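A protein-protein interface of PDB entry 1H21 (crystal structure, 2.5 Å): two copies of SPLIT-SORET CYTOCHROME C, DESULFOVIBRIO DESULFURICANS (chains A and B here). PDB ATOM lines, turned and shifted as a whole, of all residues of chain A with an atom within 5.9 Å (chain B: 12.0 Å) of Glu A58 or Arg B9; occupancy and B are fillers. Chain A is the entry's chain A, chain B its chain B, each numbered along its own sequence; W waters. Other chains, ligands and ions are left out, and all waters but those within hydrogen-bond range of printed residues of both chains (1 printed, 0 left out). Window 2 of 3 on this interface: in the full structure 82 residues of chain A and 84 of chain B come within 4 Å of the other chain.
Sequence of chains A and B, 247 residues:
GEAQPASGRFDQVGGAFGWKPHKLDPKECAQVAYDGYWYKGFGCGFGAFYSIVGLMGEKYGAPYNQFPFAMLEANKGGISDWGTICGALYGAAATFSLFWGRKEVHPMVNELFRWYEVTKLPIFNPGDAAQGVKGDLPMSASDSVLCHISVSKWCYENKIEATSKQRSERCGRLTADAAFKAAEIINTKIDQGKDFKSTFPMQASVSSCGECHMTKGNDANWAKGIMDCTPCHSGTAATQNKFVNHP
OH of Tyr A50 is in hydrogen-bond range of N of Phe B10 (2.9 Å). The guanidinium group (NH2) of Arg B9 lies within salt-bridge range of the side-chain carboxylate (OE1) of Glu A58 (2.8 Å).
O of Tyr A50 is in hydrogen-bond range of N of Leu A55 (3.1 Å). OE2 of Glu A58 is in hydrogen-bond range of OH of Tyr A50, 2.7 Å away. O of Gly A61 lies close to OD1 of Asn A65 (3.4 Å).
Val A32 touches Arg B9 (CG2 to NH1, 3.8 Å). Val A32 touches Phe B10. Asp A35 touches Phe B10 (C to CZ, 3.9 Å). CE2 of Tyr A39 touches CB of Phe B10 (3.6 Å). Tyr A50 touches Arg B9 (OH to CA, 3.5 Å). Leu A55 touches Arg B9 (CD2 to NH2, 3.4 Å). CG2 of Val B13 touches O of Asn A65, at 3.3 Å.
Printed residues of chain B within 4 Å of Val A32: Arg B9 and Phe B10. Of the printed residues of chain B, Tyr A39 touches Phe B10. Of the printed residues of chain B, Tyr A50 touches Arg B9 and Phe B10. No residue of chain B comes within 4 Å of Gly A54. Met A56 touches none of the printed residues of chain B. Glu A58 touches one residue of chain B. No residue of chain B comes within 4 Å of Lys A59. No residue of chain B comes within 4 Å of Gly A61. Of chain A, only Val A32 (3.8 Å), Tyr A50 (3.5 Å), Leu A55 (3.4 Å) and Glu A58 (2.8 Å) come within 4 Å of Arg B9. Printed residues of chain A within 4 Å of Phe B10: Val A32 (3.7 Å), Asp A35 (3.9 Å), Tyr A39 (3.6 Å) and Tyr A50 (2.9 Å). Asp B11 touches none of the printed residues of chain A. The nearest residue of chain A that does not touch Arg B9 is Glu A28 (4.2 Å). The nearest printed residue of chain B that does not touch Asp A35 is Arg B9 (5.4 Å).
Of the 8 printed residues of chain B, 3 touch a printed residue of chain A. Printed residues of chain B that touch a printed residue of chain A: Arg B9, Phe B10 and Val B13. Hydrophobic or aromatic side chains of chain B within 4 Å of the printed part of chain A: Phe B10 and Val B13. Along chain B the printed residues that touch a printed residue of chain A span positions 9 to 13. Hydrophobic or aromatic side chains of chain A that line the printed part of chain B: Val A32, Tyr A39, Tyr A50 and Leu A55. Among the printed residues, 9 pairs touch across the chains. Among the printed residues, Asp or Glu carboxylates within 4 Å of a Lys or Arg side-chain nitrogen of the other chain: Glu A58 with Arg B9 (2.8 Å).
No position is printed for both chains. Of the 9 pairs that touch across the chains among the printed residues, none has its exchanged pair printed and touching as well.
Water W1 lies within hydrogen-bond range of the side-chain carboxylate of Asp A35 (2.7 Å) and the guanidinium group of Arg B9 (3.0 Å).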
ATOM      1  N   GLU A  28       1.155  -9.700   0.272  1.00  0.00           N
ATOM      2  CA  GLU A  28       2.335  -8.911  -0.058  1.00  0.00           C
ATOM      3  C   GLU A  28       1.884  -7.704  -0.907  1.00  0.00           C
ATOM      4  O   GLU A  28       2.284  -6.552  -0.664  1.00  0.00           O
ATOM      5  CB  GLU A  28       3.366  -9.751  -0.831  1.00  0.00           C
ATOM      6  CG  GLU A  28       4.701  -9.008  -1.032  1.00  0.00           C
ATOM      7  CD  GLU A  28       5.674  -9.680  -2.018  1.00  0.00           C
ATOM      8  OE1 GLU A  28       5.272 -10.571  -2.822  1.00  0.00           O
ATOM      9  OE2 GLU A  28       6.866  -9.271  -2.002  1.00  0.00           O
ATOM     10  N   VAL A  32       2.500  -3.678  -0.238  1.00  0.00           N
ATOM     11  CA  VAL A  32       3.322  -2.832  -1.109  1.00  0.00           C
ATOM     12  C   VAL A  32       2.484  -1.704  -1.756  1.00  0.00           C
ATOM     13  O   VAL A  32       2.971  -0.580  -1.923  1.00  0.00           O
ATOM     14  CB  VAL A  32       4.028  -3.688  -2.194  1.00  0.00           C
ATOM     15  CG1 VAL A  32       4.925  -2.816  -3.064  1.00  0.00           C
ATOM     16  CG2 VAL A  32       4.834  -4.782  -1.529  1.00  0.00           C
ATOM     17  N   ASP A  35       2.062   0.984   0.694  1.00  0.00           N
ATOM     18  CA  ASP A  35       3.330   1.714   0.811  1.00  0.00           C
ATOM     19  C   ASP A  35       3.564   2.573  -0.428  1.00  0.00           C
ATOM     20  O   ASP A  35       3.953   3.746  -0.345  1.00  0.00           O
ATOM     21  CB  ASP A  35       4.507   0.736   0.990  1.00  0.00           C
ATOM     22  CG  ASP A  35       4.478   0.011   2.339  1.00  0.00           C
ATOM     23  OD1 ASP A  35       3.686   0.397   3.235  1.00  0.00           O
ATOM     24  OD2 ASP A  35       5.260  -0.957   2.507  1.00  0.00           O
ATOM     25  N   TYR A  39       4.520   6.753  -1.299  1.00  0.00           N
ATOM     26  CA  TYR A  39       5.793   7.054  -1.957  1.00  0.00           C
ATOM     27  C   TYR A  39       5.775   8.268  -2.882  1.00  0.00           C
ATOM     28  O   TYR A  39       5.085   8.281  -3.902  1.00  0.00           O
ATOM     29  CB  TYR A  39       6.300   5.829  -2.709  1.00  0.00           C
ATOM     30  CG  TYR A  39       7.649   6.035  -3.355  1.00  0.00           C
ATOM     31  CD1 TYR A  39       8.817   6.045  -2.595  1.00  0.00           C
ATOM     32  CD2 TYR A  39       7.755   6.221  -4.730  1.00  0.00           C
ATOM     33  CE1 TYR A  39      10.069   6.240  -3.194  1.00  0.00           C
ATOM     34  CE2 TYR A  39       8.986   6.416  -5.339  1.00  0.00           C
ATOM     35  CZ  TYR A  39      10.137   6.427  -4.568  1.00  0.00           C
ATOM     36  OH  TYR A  39      11.344   6.647  -5.194  1.00  0.00           O
ATOM     37  N   TYR A  50       2.164  -0.744  -9.188  1.00  0.00           N
ATOM     38  CA  TYR A  50       3.441  -1.264  -8.753  1.00  0.00           C
ATOM     39  C   TYR A  50       3.336  -2.563  -7.950  1.00  0.00           C
ATOM     40  O   TYR A  50       4.085  -3.500  -8.207  1.00  0.00           O
ATOM     41  CB  TYR A  50       4.212  -0.228  -7.952  1.00  0.00           C
ATOM     42  CG  TYR A  50       5.634  -0.655  -7.694  1.00  0.00           C
ATOM     43  CD1 TYR A  50       6.663  -0.222  -8.522  1.00  0.00           C
ATOM     44  CD2 TYR A  50       5.959  -1.494  -6.622  1.00  0.00           C
ATOM     45  CE1 TYR A  50       7.981  -0.604  -8.294  1.00  0.00           C
ATOM     46  CE2 TYR A  50       7.280  -1.886  -6.387  1.00  0.00           C
ATOM     47  CZ  TYR A  50       8.280  -1.429  -7.232  1.00  0.00           C
ATOM     48  OH  TYR A  50       9.593  -1.756  -7.010  1.00  0.00           O
ATOM     49  N   VAL A  53       2.963  -5.240 -11.072  1.00  0.00           N
ATOM     50  CA  VAL A  53       4.036  -5.301 -12.060  1.00  0.00           C
ATOM     51  C   VAL A  53       5.360  -4.924 -11.424  1.00  0.00           C
ATOM     52  O   VAL A  53       6.414  -5.394 -11.849  1.00  0.00           O
ATOM     53  CB  VAL A  53       3.724  -4.375 -13.250  1.00  0.00           C
ATOM     54  CG1 VAL A  53       4.850  -4.387 -14.266  1.00  0.00           C
ATOM     55  CG2 VAL A  53       2.402  -4.791 -13.899  1.00  0.00           C
ATOM     56  N   GLY A  54       5.300  -4.094 -10.390  1.00  0.00           N
ATOM     57  CA  GLY A  54       6.511  -3.680  -9.702  1.00  0.00           C
ATOM     58  C   GLY A  54       7.123  -4.853  -8.946  1.00  0.00           C
ATOM     59  O   GLY A  54       8.345  -5.041  -8.963  1.00  0.00           O
ATOM     60  N   LEU A  55       6.282  -5.632  -8.271  1.00  0.00           N
ATOM     61  CA  LEU A  55       6.771  -6.795  -7.539  1.00  0.00           C
ATOM     62  C   LEU A  55       7.232  -7.891  -8.501  1.00  0.00           C
ATOM     63  O   LEU A  55       8.176  -8.608  -8.203  1.00  0.00           O
ATOM     64  CB  LEU A  55       5.727  -7.323  -6.557  1.00  0.00           C
ATOM     65  CG  LEU A  55       5.409  -6.362  -5.412  1.00  0.00           C
ATOM     66  CD1 LEU A  55       4.613  -7.123  -4.404  1.00  0.00           C
ATOM     67  CD2 LEU A  55       6.680  -5.810  -4.780  1.00  0.00           C
ATOM     68  N   MET A  56       6.577  -8.027  -9.649  1.00  0.00           N
ATOM     69  CA  MET A  56       7.015  -9.012 -10.640  1.00  0.00           C
ATOM     70  C   MET A  56       8.400  -8.586 -11.168  1.00  0.00           C
ATOM     71  O   MET A  56       9.225  -9.429 -11.518  1.00  0.00           O
ATOM     72  CB  MET A  56       6.032  -9.115 -11.819  1.00  0.00           C
ATOM     73  CG  MET A  56       4.724  -9.778 -11.478  1.00  0.00           C
ATOM     74  SD  MET A  56       3.869 -10.227 -12.973  1.00  0.00           S
ATOM     75  CE  MET A  56       2.224 -10.635 -12.315  1.00  0.00           C
ATOM     76  N   GLY A  57       8.653  -7.280 -11.216  1.00  0.00           N
ATOM     77  CA  GLY A  57       9.937  -6.788 -11.686  1.00  0.00           C
ATOM     78  C   GLY A  57      11.070  -7.081 -10.712  1.00  0.00           C
ATOM     79  O   GLY A  57      12.158  -7.482 -11.136  1.00  0.00           O
ATOM     80  N   GLU A  58      10.829  -6.849  -9.422  1.00  0.00           N
ATOM     81  CA  GLU A  58      11.817  -7.110  -8.374  1.00  0.00           C
ATOM     82  C   GLU A  58      12.233  -8.592  -8.324  1.00  0.00           C
ATOM     83  O   GLU A  58      13.417  -8.900  -8.146  1.00  0.00           O
ATOM     84  CB  GLU A  58      11.261  -6.704  -7.005  1.00  0.00           C
ATOM     85  CG  GLU A  58      11.056  -5.205  -6.808  1.00  0.00           C
ATOM     86  CD  GLU A  58      10.491  -4.859  -5.421  1.00  0.00           C
ATOM     87  OE1 GLU A  58      10.280  -5.777  -4.586  1.00  0.00           O
ATOM     88  OE2 GLU A  58      10.250  -3.660  -5.155  1.00  0.00           O
ATOM     89  N   LYS A  59      11.260  -9.491  -8.492  1.00  0.00           N
ATOM     90  CA  LYS A  59      11.500 -10.935  -8.452  1.00  0.00           C
ATOM     91  C   LYS A  59      11.964 -11.580  -9.771  1.00  0.00           C
ATOM     92  O   LYS A  59      12.837 -12.450  -9.776  1.00  0.00           O
ATOM     93  CB  LYS A  59      10.241 -11.670  -7.942  1.00  0.00           C
ATOM     94  CG  LYS A  59       9.816 -11.327  -6.495  1.00  0.00           C
ATOM     95  CD  LYS A  59       8.417 -11.901  -6.179  1.00  0.00           C
ATOM     96  CE  LYS A  59       7.983 -11.700  -4.714  1.00  0.00           C
ATOM     97  NZ  LYS A  59       8.209 -10.310  -4.228  1.00  0.00           N
ATOM     98  N   TYR A  60      11.397 -11.165 -10.894  1.00  0.00           N
ATOM     99  CA  TYR A  60      11.758 -11.782 -12.166  1.00  0.00           C
ATOM    100  C   TYR A  60      12.410 -10.879 -13.206  1.00  0.00           C
ATOM    101  O   TYR A  60      12.524 -11.281 -14.372  1.00  0.00           O
ATOM    102  CB  TYR A  60      10.532 -12.447 -12.802  1.00  0.00           C
ATOM    103  CG  TYR A  60       9.671 -13.234 -11.841  1.00  0.00           C
ATOM    104  CD1 TYR A  60       8.538 -12.663 -11.258  1.00  0.00           C
ATOM    105  CD2 TYR A  60       9.974 -14.550 -11.527  1.00  0.00           C
ATOM    106  CE1 TYR A  60       7.721 -13.387 -10.380  1.00  0.00           C
ATOM    107  CE2 TYR A  60       9.161 -15.290 -10.648  1.00  0.00           C
ATOM    108  CZ  TYR A  60       8.038 -14.697 -10.079  1.00  0.00           C
ATOM    109  OH  TYR A  60       7.236 -15.398  -9.194  1.00  0.00           O
ATOM    110  N   GLY A  61      12.816  -9.673 -12.813  1.00  0.00           N
ATOM    111  CA  GLY A  61      13.460  -8.766 -13.754  1.00  0.00           C
ATOM    112  C   GLY A  61      12.599  -8.262 -14.911  1.00  0.00           C
ATOM    113  O   GLY A  61      11.436  -7.907 -14.723  1.00  0.00           O
ATOM    114  N   ASN A  65      10.394  -4.980 -14.913  1.00  0.00           N
ATOM    115  CA  ASN A  65      11.183  -3.931 -14.293  1.00  0.00           C
ATOM    116  C   ASN A  65      11.671  -2.796 -15.210  1.00  0.00           C
ATOM    117  O   ASN A  65      12.472  -1.933 -14.789  1.00  0.00           O
ATOM    118  CB  ASN A  65      12.329  -4.535 -13.457  1.00  0.00           C
ATOM    119  CG  ASN A  65      13.527  -5.003 -14.301  1.00  0.00           C
ATOM    120  OD1 ASN A  65      13.434  -5.238 -15.524  1.00  0.00           O
ATOM    121  ND2 ASN A  65      14.669  -5.143 -13.629  1.00  0.00           N
ATOM    122  N   GLY B   8      16.194   0.975  -6.507  1.00  0.00           N
ATOM    123  CA  GLY B   8      15.473   0.648  -5.227  1.00  0.00           C
ATOM    124  C   GLY B   8      14.014   0.349  -5.515  1.00  0.00           C
ATOM    125  O   GLY B   8      13.569   0.515  -6.652  1.00  0.00           O
ATOM    126  N   ARG B   9      13.282  -0.135  -4.512  1.00  0.00           N
ATOM    127  CA  ARG B   9      11.855  -0.439  -4.671  1.00  0.00           C
ATOM    128  C   ARG B   9      11.164   0.880  -4.948  1.00  0.00           C
ATOM    129  O   ARG B   9      11.506   1.892  -4.319  1.00  0.00           O
ATOM    130  CB  ARG B   9      11.290  -1.065  -3.388  1.00  0.00           C
ATOM    131  CG  ARG B   9       9.777  -1.056  -3.295  1.00  0.00           C
ATOM    132  CD  ARG B   9       9.260  -1.915  -2.153  1.00  0.00           C
ATOM    133  NE  ARG B   9       9.255  -3.333  -2.517  1.00  0.00           N
ATOM    134  CZ  ARG B   9       8.861  -4.335  -1.724  1.00  0.00           C
ATOM    135  NH1 ARG B   9       8.428  -4.091  -0.487  1.00  0.00           N
ATOM    136  NH2 ARG B   9       8.857  -5.586  -2.186  1.00  0.00           N
ATOM    137  N   PHE B  10      10.226   0.862  -5.905  1.00  0.00           N
ATOM    138  CA  PHE B  10       9.443   2.032  -6.327  1.00  0.00           C
ATOM    139  C   PHE B  10      10.122   2.950  -7.358  1.00  0.00           C
ATOM    140  O   PHE B  10       9.442   3.802  -7.933  1.00  0.00           O
ATOM    141  CB  PHE B  10       8.977   2.869  -5.122  1.00  0.00           C
ATOM    142  CG  PHE B  10       8.046   2.141  -4.195  1.00  0.00           C
ATOM    143  CD1 PHE B  10       8.044   2.417  -2.837  1.00  0.00           C
ATOM    144  CD2 PHE B  10       7.176   1.173  -4.683  1.00  0.00           C
ATOM    145  CE1 PHE B  10       7.197   1.747  -1.973  1.00  0.00           C
ATOM    146  CE2 PHE B  10       6.312   0.482  -3.821  1.00  0.00           C
ATOM    147  CZ  PHE B  10       6.328   0.775  -2.459  1.00  0.00           C
ATOM    148  N   ASP B  11      11.440   2.835  -7.552  1.00  0.00           N
ATOM    149  CA  ASP B  11      12.114   3.676  -8.540  1.00  0.00           C
ATOM    150  C   ASP B  11      11.959   3.004  -9.893  1.00  0.00           C
ATOM    151  O   ASP B  11      11.451   1.888  -9.959  1.00  0.00           O
ATOM    152  CB  ASP B  11      13.597   3.928  -8.214  1.00  0.00           C
ATOM    153  CG  ASP B  11      14.201   5.082  -9.061  1.00  0.00           C
ATOM    154  OD1 ASP B  11      13.578   6.177  -9.160  1.00  0.00           O
ATOM    155  OD2 ASP B  11      15.298   4.894  -9.638  1.00  0.00           O
ATOM    156  N   GLN B  12      12.395   3.666 -10.965  1.00  0.00           N
ATOM    157  CA  GLN B  12      12.225   3.124 -12.311  1.00  0.00           C
ATOM    158  C   GLN B  12      13.391   3.477 -13.182  1.00  0.00           C
ATOM    159  O   GLN B  12      14.112   4.438 -12.911  1.00  0.00           O
ATOM    160  CB  GLN B  12      10.966   3.704 -12.973  1.00  0.00           C
ATOM    161  CG  GLN B  12      11.086   5.189 -13.341  1.00  0.00           C
ATOM    162  CD  GLN B  12       9.746   5.834 -13.609  1.00  0.00           C
ATOM    163  OE1 GLN B  12       9.472   6.328 -14.714  1.00  0.00           O
ATOM    164  NE2 GLN B  12       8.884   5.809 -12.602  1.00  0.00           N
ATOM    165  N   VAL B  13      13.518   2.754 -14.289  1.00  0.00           N
ATOM    166  CA  VAL B  13      14.601   2.998 -15.227  1.00  0.00           C
ATOM    167  C   VAL B  13      14.421   4.405 -15.830  1.00  0.00           C
ATOM    168  O   VAL B  13      13.401   4.708 -16.464  1.00  0.00           O
ATOM    169  CB  VAL B  13      14.645   1.912 -16.348  1.00  0.00           C
ATOM    170  CG1 VAL B  13      15.949   2.048 -17.139  1.00  0.00           C
ATOM    171  CG2 VAL B  13      14.545   0.504 -15.747  1.00  0.00           C
ATOM    172  N   GLY B  15      14.452   7.198 -13.885  1.00  0.00           N
ATOM    173  CA  GLY B  15      13.952   8.069 -12.840  1.00  0.00           C
ATOM    174  C   GLY B  15      12.514   8.444 -13.168  1.00  0.00           C
ATOM    175  O   GLY B  15      12.089   8.351 -14.329  1.00  0.00           O
ATOM    176  N   ALA B  16      11.737   8.802 -12.145  1.00  0.00           N
ATOM    177  CA  ALA B  16      10.340   9.214 -12.336  1.00  0.00           C
ATOM    178  C   ALA B  16      10.341  10.451 -13.243  1.00  0.00           C
ATOM    179  O   ALA B  16      11.159  11.361 -13.041  1.00  0.00           O
ATOM    180  CB  ALA B  16       9.710   9.565 -10.992  1.00  0.00           C
HETATM  181  O   HOH W   1       6.972  -1.731   0.563  1.00  0.00           O
